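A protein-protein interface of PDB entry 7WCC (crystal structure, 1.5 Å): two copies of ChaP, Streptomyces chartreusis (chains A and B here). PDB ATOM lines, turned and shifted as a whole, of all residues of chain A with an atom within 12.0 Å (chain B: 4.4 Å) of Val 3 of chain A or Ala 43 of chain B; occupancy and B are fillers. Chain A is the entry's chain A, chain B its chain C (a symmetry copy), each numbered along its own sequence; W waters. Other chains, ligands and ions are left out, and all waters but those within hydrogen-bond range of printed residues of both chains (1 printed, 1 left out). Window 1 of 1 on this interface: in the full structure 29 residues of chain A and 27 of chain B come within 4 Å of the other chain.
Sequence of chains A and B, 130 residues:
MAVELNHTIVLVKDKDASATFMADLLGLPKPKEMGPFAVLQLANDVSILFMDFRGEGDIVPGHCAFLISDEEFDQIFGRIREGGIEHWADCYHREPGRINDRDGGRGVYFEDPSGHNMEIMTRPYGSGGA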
ATOM      1  N   ALA A   2       5.478 -20.805   5.111  1.00  0.00           N
ATOM      2  CA  ALA A   2       4.363 -21.222   5.950  1.00  0.00           C
ATOM      3  C   ALA A   2       4.833 -21.412   7.394  1.00  0.00           C
ATOM      4  O   ALA A   2       5.722 -22.216   7.669  1.00  0.00           O
ATOM      5  CB  ALA A   2       3.744 -22.485   5.402  1.00  0.00           C
ATOM      6  N   VAL A   3       4.208 -20.684   8.314  1.00  0.00           N
ATOM      7  CA  VAL A   3       4.623 -20.663   9.714  1.00  0.00           C
ATOM      8  C   VAL A   3       4.016 -21.855  10.442  1.00  0.00           C
ATOM      9  O   VAL A   3       2.791 -22.007  10.487  1.00  0.00           O
ATOM     10  CB  VAL A   3       4.213 -19.345  10.387  1.00  0.00           C
ATOM     11  CG1 VAL A   3       4.632 -19.341  11.850  1.00  0.00           C
ATOM     12  CG2 VAL A   3       4.816 -18.161   9.642  1.00  0.00           C
ATOM     13  N   GLU A   4       4.871 -22.699  11.015  1.00  0.00           N
ATOM     14  CA  GLU A   4       4.444 -23.899  11.725  1.00  0.00           C
ATOM     15  C   GLU A   4       4.629 -23.713  13.225  1.00  0.00           C
ATOM     16  O   GLU A   4       5.590 -23.076  13.662  1.00  0.00           O
ATOM     17  CB  GLU A   4       5.253 -25.118  11.271  1.00  0.00           C
ATOM     18  CG  GLU A   4       5.130 -25.427   9.793  1.00  0.00           C
ATOM     19  CD  GLU A   4       5.955 -26.630   9.371  1.00  0.00           C
ATOM     20  OE1 GLU A   4       6.737 -27.148  10.198  1.00  0.00           O
ATOM     21  OE2 GLU A   4       5.835 -27.046   8.200  1.00  0.00           O
ATOM     22  N   LEU A   5       3.710 -24.265  14.013  1.00  0.00           N
ATOM     23  CA  LEU A   5       3.936 -24.402  15.449  1.00  0.00           C
ATOM     24  C   LEU A   5       4.767 -25.659  15.668  1.00  0.00           C
ATOM     25  O   LEU A   5       4.308 -26.768  15.373  1.00  0.00           O
ATOM     26  CB  LEU A   5       2.616 -24.465  16.216  1.00  0.00           C
ATOM     27  CG  LEU A   5       2.743 -24.679  17.726  1.00  0.00           C
ATOM     28  CD1 LEU A   5       3.455 -23.514  18.395  1.00  0.00           C
ATOM     29  CD2 LEU A   5       1.365 -24.894  18.351  1.00  0.00           C
ATOM     30  N   ASN A   6       5.997 -25.489  16.156  1.00  0.00           N
ATOM     31  CA  ASN A   6       6.938 -26.600  16.267  1.00  0.00           C
ATOM     32  C   ASN A   6       6.905 -27.291  17.627  1.00  0.00           C
ATOM     33  O   ASN A   6       7.013 -28.520  17.692  1.00  0.00           O
ATOM     34  CB  ASN A   6       8.356 -26.109  15.972  1.00  0.00           C
ATOM     35  CG  ASN A   6       9.374 -27.232  15.984  1.00  0.00           C
ATOM     36  OD1 ASN A   6      10.052 -27.457  16.984  1.00  0.00           O
ATOM     37  ND2 ASN A   6       9.477 -27.952  14.866  1.00  0.00           N
ATOM     38  N   HIS A   7       6.783 -26.541  18.721  1.00  0.00           N
ATOM     39  CA  HIS A   7       6.647 -27.181  20.021  1.00  0.00           C
ATOM     40  C   HIS A   7       6.021 -26.207  21.004  1.00  0.00           C
ATOM     41  O   HIS A   7       6.001 -24.993  20.788  1.00  0.00           O
ATOM     42  CB  HIS A   7       7.985 -27.732  20.558  1.00  0.00           C
ATOM     43  CG  HIS A   7       9.107 -26.735  20.649  1.00  0.00           C
ATOM     44  ND1 HIS A   7       9.974 -26.494  19.606  1.00  0.00           N
ATOM     45  CD2 HIS A   7       9.553 -25.986  21.687  1.00  0.00           C
ATOM     46  CE1 HIS A   7      10.890 -25.619  19.986  1.00  0.00           C
ATOM     47  NE2 HIS A   7      10.653 -25.289  21.244  1.00  0.00           N
ATOM     48  N   ALA A  43       2.195 -36.149  14.852  1.00  0.00           N
ATOM     49  CA  ALA A  43       2.500 -36.451  13.458  1.00  0.00           C
ATOM     50  C   ALA A  43       2.678 -35.196  12.611  1.00  0.00           C
ATOM     51  O   ALA A  43       3.391 -35.234  11.598  1.00  0.00           O
ATOM     52  CB  ALA A  43       1.400 -37.330  12.867  1.00  0.00           C
ATOM     53  N   ASN A  44       2.039 -34.090  12.984  1.00  0.00           N
ATOM     54  CA  ASN A  44       2.055 -32.881  12.156  1.00  0.00           C
ATOM     55  C   ASN A  44       3.167 -31.913  12.562  1.00  0.00           C
ATOM     56  O   ASN A  44       2.959 -30.706  12.674  1.00  0.00           O
ATOM     57  CB  ASN A  44       0.687 -32.204  12.187  1.00  0.00           C
ATOM     58  CG  ASN A  44       0.168 -31.953  13.598  1.00  0.00           C
ATOM     59  OD1 ASN A  44       0.410 -32.732  14.522  1.00  0.00           O
ATOM     60  ND2 ASN A  44      -0.572 -30.860  13.761  1.00  0.00           N
ATOM     61  N   ASP A  45       4.371 -32.449  12.763  1.00  0.00           N
ATOM     62  CA  ASP A  45       5.578 -31.642  12.974  1.00  0.00           C
ATOM     63  C   ASP A  45       5.433 -30.708  14.174  1.00  0.00           C
ATOM     64  O   ASP A  45       5.905 -29.568  14.159  1.00  0.00           O
ATOM     65  CB  ASP A  45       5.940 -30.847  11.715  1.00  0.00           C
ATOM     66  CG  ASP A  45       6.286 -31.742  10.535  1.00  0.00           C
ATOM     67  OD1 ASP A  45       6.745 -32.880  10.762  1.00  0.00           O
ATOM     68  OD2 ASP A  45       6.098 -31.305   9.381  1.00  0.00           O
ATOM     69  N   VAL A  46       4.790 -31.194  15.229  1.00  0.00           N
ATOM     70  CA  VAL A  46       4.673 -30.442  16.473  1.00  0.00           C
ATOM     71  C   VAL A  46       4.847 -31.414  17.630  1.00  0.00           C
ATOM     72  O   VAL A  46       4.410 -32.568  17.557  1.00  0.00           O
ATOM     73  CB  VAL A  46       3.332 -29.678  16.554  1.00  0.00           C
ATOM     74  CG1 VAL A  46       2.156 -30.633  16.477  1.00  0.00           C
ATOM     75  CG2 VAL A  46       3.265 -28.814  17.816  1.00  0.00           C
ATOM     76  N   LEU A  67      -6.285 -34.678  16.553  1.00  0.00           N
ATOM     77  CA  LEU A  67      -7.025 -35.190  15.408  1.00  0.00           C
ATOM     78  C   LEU A  67      -6.444 -36.545  15.032  1.00  0.00           C
ATOM     79  O   LEU A  67      -5.234 -36.671  14.819  1.00  0.00           O
ATOM     80  CB  LEU A  67      -6.951 -34.222  14.224  1.00  0.00           C
ATOM     81  CG  LEU A  67      -7.669 -34.663  12.945  1.00  0.00           C
ATOM     82  CD1 LEU A  67      -9.167 -34.722  13.166  1.00  0.00           C
ATOM     83  CD2 LEU A  67      -7.332 -33.744  11.779  1.00  0.00           C
ATOM     84  N   PRO A 124     -12.016 -32.547  11.469  1.00  0.00           N
ATOM     85  CA  PRO A 124     -11.724 -31.164  11.861  1.00  0.00           C
ATOM     86  C   PRO A 124     -12.982 -30.441  12.320  1.00  0.00           C
ATOM     87  O   PRO A 124     -14.075 -30.659  11.794  1.00  0.00           O
ATOM     88  CB  PRO A 124     -11.151 -30.548  10.581  1.00  0.00           C
ATOM     89  CG  PRO A 124     -10.594 -31.713   9.832  1.00  0.00           C
ATOM     90  CD  PRO A 124     -11.551 -32.839  10.102  1.00  0.00           C
ATOM     91  N   LEU B  26       3.829 -12.482  12.790  1.00  0.00           N
ATOM     92  CA  LEU B  26       4.143 -13.659  11.993  1.00  0.00           C
ATOM     93  C   LEU B  26       3.702 -13.533  10.538  1.00  0.00           C
ATOM     94  O   LEU B  26       3.994 -14.433   9.744  1.00  0.00           O
ATOM     95  CB  LEU B  26       3.509 -14.900  12.626  1.00  0.00           C
ATOM     96  CG  LEU B  26       4.001 -15.246  14.035  1.00  0.00           C
ATOM     97  CD1 LEU B  26       3.188 -16.395  14.614  1.00  0.00           C
ATOM     98  CD2 LEU B  26       5.487 -15.576  14.029  1.00  0.00           C
ATOM     99  N   LEU B  42      -1.945 -22.023  12.353  1.00  0.00           N
ATOM    100  CA  LEU B  42      -0.620 -22.272  11.802  1.00  0.00           C
ATOM    101  C   LEU B  42      -0.707 -23.247  10.630  1.00  0.00           C
ATOM    102  O   LEU B  42      -1.739 -23.874  10.374  1.00  0.00           O
ATOM    103  CB  LEU B  42       0.336 -22.792  12.880  1.00  0.00           C
ATOM    104  CG  LEU B  42       0.713 -21.819  14.006  1.00  0.00           C
ATOM    105  CD1 LEU B  42       0.901 -20.394  13.476  1.00  0.00           C
ATOM    106  CD2 LEU B  42      -0.296 -21.849  15.150  1.00  0.00           C
ATOM    107  N   ALA B  43       0.404 -23.358   9.901  1.00  0.00           N
ATOM    108  CA  ALA B  43       0.381 -24.057   8.621  1.00  0.00           C
ATOM    109  C   ALA B  43       0.295 -25.568   8.781  1.00  0.00           C
ATOM    110  O   ALA B  43      -0.232 -26.251   7.894  1.00  0.00           O
ATOM    111  CB  ALA B  43       1.620 -23.694   7.812  1.00  0.00           C
ATOM    112  N   ASN B  44       0.809 -26.109   9.882  1.00  0.00           N
ATOM    113  CA  ASN B  44       0.886 -27.561  10.041  1.00  0.00           C
ATOM    114  C   ASN B  44      -0.339 -28.119  10.762  1.00  0.00           C
ATOM    115  O   ASN B  44      -0.239 -28.934  11.678  1.00  0.00           O
ATOM    116  CB  ASN B  44       2.183 -27.953  10.745  1.00  0.00           C
ATOM    117  CG  ASN B  44       2.423 -27.189  12.038  1.00  0.00           C
ATOM    118  OD1 ASN B  44       2.080 -26.012  12.162  1.00  0.00           O
ATOM    119  ND2 ASN B  44       3.042 -27.861  13.005  1.00  0.00           N
ATOM    120  N   ASP B  45      -1.518 -27.671  10.326  1.00  0.00           N
ATOM    121  CA  ASP B  45      -2.797 -28.233  10.770  1.00  0.00           C
ATOM    122  C   ASP B  45      -2.946 -28.158  12.288  1.00  0.00           C
ATOM    123  O   ASP B  45      -3.458 -29.079  12.928  1.00  0.00           O
ATOM    124  CB  ASP B  45      -2.968 -29.671  10.274  1.00  0.00           C
ATOM    125  CG  ASP B  45      -3.011 -29.759   8.760  1.00  0.00           C
ATOM    126  OD1 ASP B  45      -3.415 -28.766   8.121  1.00  0.00           O
ATOM    127  OD2 ASP B  45      -2.639 -30.817   8.212  1.00  0.00           O
ATOM    128  N   PHE B  66       7.919 -21.504  16.920  1.00  0.00           N
ATOM    129  CA  PHE B  66       7.449 -21.571  15.546  1.00  0.00           C
ATOM    130  C   PHE B  66       8.627 -21.818  14.616  1.00  0.00           C
ATOM    131  O   PHE B  66       9.663 -21.154  14.728  1.00  0.00           O
ATOM    132  CB  PHE B  66       6.723 -20.280  15.153  1.00  0.00           C
ATOM    133  CG  PHE B  66       5.576 -19.936  16.061  1.00  0.00           C
ATOM    134  CD1 PHE B  66       4.299 -20.411  15.803  1.00  0.00           C
ATOM    135  CD2 PHE B  66       5.780 -19.148  17.181  1.00  0.00           C
ATOM    136  CE1 PHE B  66       3.241 -20.101  16.644  1.00  0.00           C
ATOM    137  CE2 PHE B  66       4.730 -18.836  18.028  1.00  0.00           C
ATOM    138  CZ  PHE B  66       3.457 -19.314  17.758  1.00  0.00           C
ATOM    139  N   LEU B  67       8.466 -22.776  13.708  1.00  0.00           N
ATOM    140  CA  LEU B  67       9.464 -23.084  12.693  1.00  0.00           C
ATOM    141  C   LEU B  67       9.079 -22.377  11.400  1.00  0.00           C
ATOM    142  O   LEU B  67       7.950 -22.531  10.917  1.00  0.00           O
ATOM    143  CB  LEU B  67       9.561 -24.594  12.489  1.00  0.00           C
ATOM    144  CG  LEU B  67      10.547 -25.064  11.424  1.00  0.00           C
ATOM    145  CD1 LEU B  67      11.964 -24.723  11.833  1.00  0.00           C
ATOM    146  CD2 LEU B  67      10.397 -26.558  11.217  1.00  0.00           C
ATOM    147  N   ILE B  68      10.002 -21.578  10.861  1.00  0.00           N
ATOM    148  CA  ILE B  68       9.731 -20.742   9.700  1.00  0.00           C
ATOM    149  C   ILE B  68      10.888 -20.858   8.714  1.00  0.00           C
ATOM    150  O   ILE B  68      11.978 -21.330   9.042  1.00  0.00           O
ATOM    151  CB  ILE B  68       9.498 -19.266  10.095  1.00  0.00           C
ATOM    152  CG1 ILE B  68      10.750 -18.685  10.751  1.00  0.00           C
ATOM    153  CG2 ILE B  68       8.298 -19.139  11.032  1.00  0.00           C
ATOM    154  CD1 ILE B  68      10.611 -17.231  11.159  1.00  0.00           C
ATOM    155  N   GLU B  72      10.958 -16.117   5.576  1.00  0.00           N
ATOM    156  CA  GLU B  72       9.993 -15.692   6.581  1.00  0.00           C
ATOM    157  C   GLU B  72      10.689 -15.078   7.788  1.00  0.00           C
ATOM    158  O   GLU B  72      10.179 -14.120   8.381  1.00  0.00           O
ATOM    159  CB  GLU B  72       9.119 -16.876   6.985  1.00  0.00           C
ATOM    160  CG  GLU B  72       8.083 -17.210   5.931  1.00  0.00           C
ATOM    161  CD  GLU B  72       7.417 -18.546   6.159  1.00  0.00           C
ATOM    162  OE1 GLU B  72       8.053 -19.444   6.750  1.00  0.00           O
ATOM    163  OE2 GLU B  72       6.256 -18.702   5.729  1.00  0.00           O
ATOM    164  N   ILE B  76       9.771 -11.559   9.410  1.00  0.00           N
ATOM    165  CA  ILE B  76       9.264 -11.487  10.778  1.00  0.00           C
ATOM    166  C   ILE B  76      10.250 -10.745  11.674  1.00  0.00           C
ATOM    167  O   ILE B  76       9.864  -9.855  12.441  1.00  0.00           O
ATOM    168  CB  ILE B  76       8.957 -12.897  11.316  1.00  0.00           C
ATOM    169  CG1 ILE B  76       7.796 -13.523  10.539  1.00  0.00           C
ATOM    170  CG2 ILE B  76       8.628 -12.840  12.801  1.00  0.00           C
ATOM    171  CD1 ILE B  76       7.651 -15.028  10.749  1.00  0.00           C
HETATM  172  O   HOH W   1       8.695 -23.857   8.248  1.00  0.00           O
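The backbone NH of Ala 2 of chain A lies close to the side-chain carboxylate of Glu 72 of chain B (3.3 Å).
O of Val 3 of chain A sits at hydrogen-bond distance from N of Ala 43 of chain B (2.8 Å).
The backbone carbonyl oxygen of Glu 4 of chain A lies within hydrogen-bond range of the backbone NH of Leu 67 of chain B (2.9 Å).
ND2 of Asn 44 of chain B is in hydrogen-bond range of O of Leu 5 of chain A (2.9 Å).
The side-chain amide nitrogen (ND2) of Asn 44 of chain A is in hydrogen-bond range of the backbone carbonyl oxygen (O) of Asn 44 of chain B (2.9 Å).
O of Asp 45 of chain B lies within hydrogen-bond range of ND2 of Asn 44 of chain A (3.5 Å).
Water W1 lies within hydrogen-bond range of O of Leu 67 of chain B and O of Ala 2 of chain A.
Asn 44 of chain B touches its own counterpart, Asn 44 of chain A.
Asn 44 of chain A touches Asp 45 of chain B, and with the chains exchanged Asp 45 of chain A touches Asn 44 of chain B.
4 positions are printed for both chains.
Of the 10 printed residues of chain B, 9 touch a printed residue of chain A.
Hydrophobic or aromatic side chains of chain B within 4 Å of the printed part of chain A: Leu 42, Ala 43, Phe 66, Leu 67 and Ile 68.
Among the printed residues, 19 pairs touch across the chains.
Among the printed residues, no Asp or Glu carboxylate lies within 4 Å of a Lys or Arg side-chain nitrogen of the other chain.
OD1 of Asn 6 of chain A lies within hydrogen-bond range of ND1 of His 7 of chain A (2.8 Å).
Ala 43 of chain B touches Ala 2 of chain A (CB to CB, 3.4 Å).
Leu 26 of chain B touches Val 3 of chain A.
N of Val 3 of chain A touches OE2 of Glu 72 of chain B (3.8 Å).
Glu 4 of chain A touches Asn 44 of chain B.
O of Glu 4 of chain A touches CA of Phe 66 of chain B (3.0 Å).
Leu 5 of chain A touches Leu 42 of chain B.
CD1 of Leu 5 of chain A touches CE1 of Phe 66 of chain B, 3.8 Å away.
Asn 6 of chain A touches Leu 67 of chain B (CB to CB, 3.98 Å).
Asn 44 of chain B touches Asp 45 of chain A.
Asn 44 of chain B touches Val 46 of chain A (ND2 to CB, 3.998 Å).
Printed residues of chain B within 4 Å of Val 3 of chain A: Leu 26 (3.8 Å), Leu 42 (3.5 Å), Ala 43 (2.8 Å), Ile 68 (3.8 Å) and Glu 72 (3.8 Å).
Ala 43 of chain B touches just these residues of chain A: Ala 2 and Val 3.
Of chain A, only Val 3 (3.5 Å) and Leu 5 (3.9 Å) come within 4 Å of Leu 42 of chain B.
Asp 45 of chain B touches one residue of chain A.
Ile 68 of chain B touches just one residue of chain A: Val 3 (3.8 Å).
Of chain A, only Ala 2 and Val 3 come within 4 Å of Glu 72 of chain B.
Printed residues of chain B within 4 Å of Ala 2 of chain A: Ala 43, Leu 67 and Glu 72.
Printed residues of chain B within 4 Å of Leu 5 of chain A: Leu 42, Asn 44 and Phe 66.
Printed residues of chain B within 4 Å of Val 46 of chain A: Asn 44 (3.998 Å).
Of the printed residues of chain B, Asn 44 of chain A touches Asn 44 (2.9 Å) and Asp 45 (3.5 Å).
The nearest printed residue of chain B that does not touch Val 3 of chain A is Leu 67 of chain B (4.001 Å).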
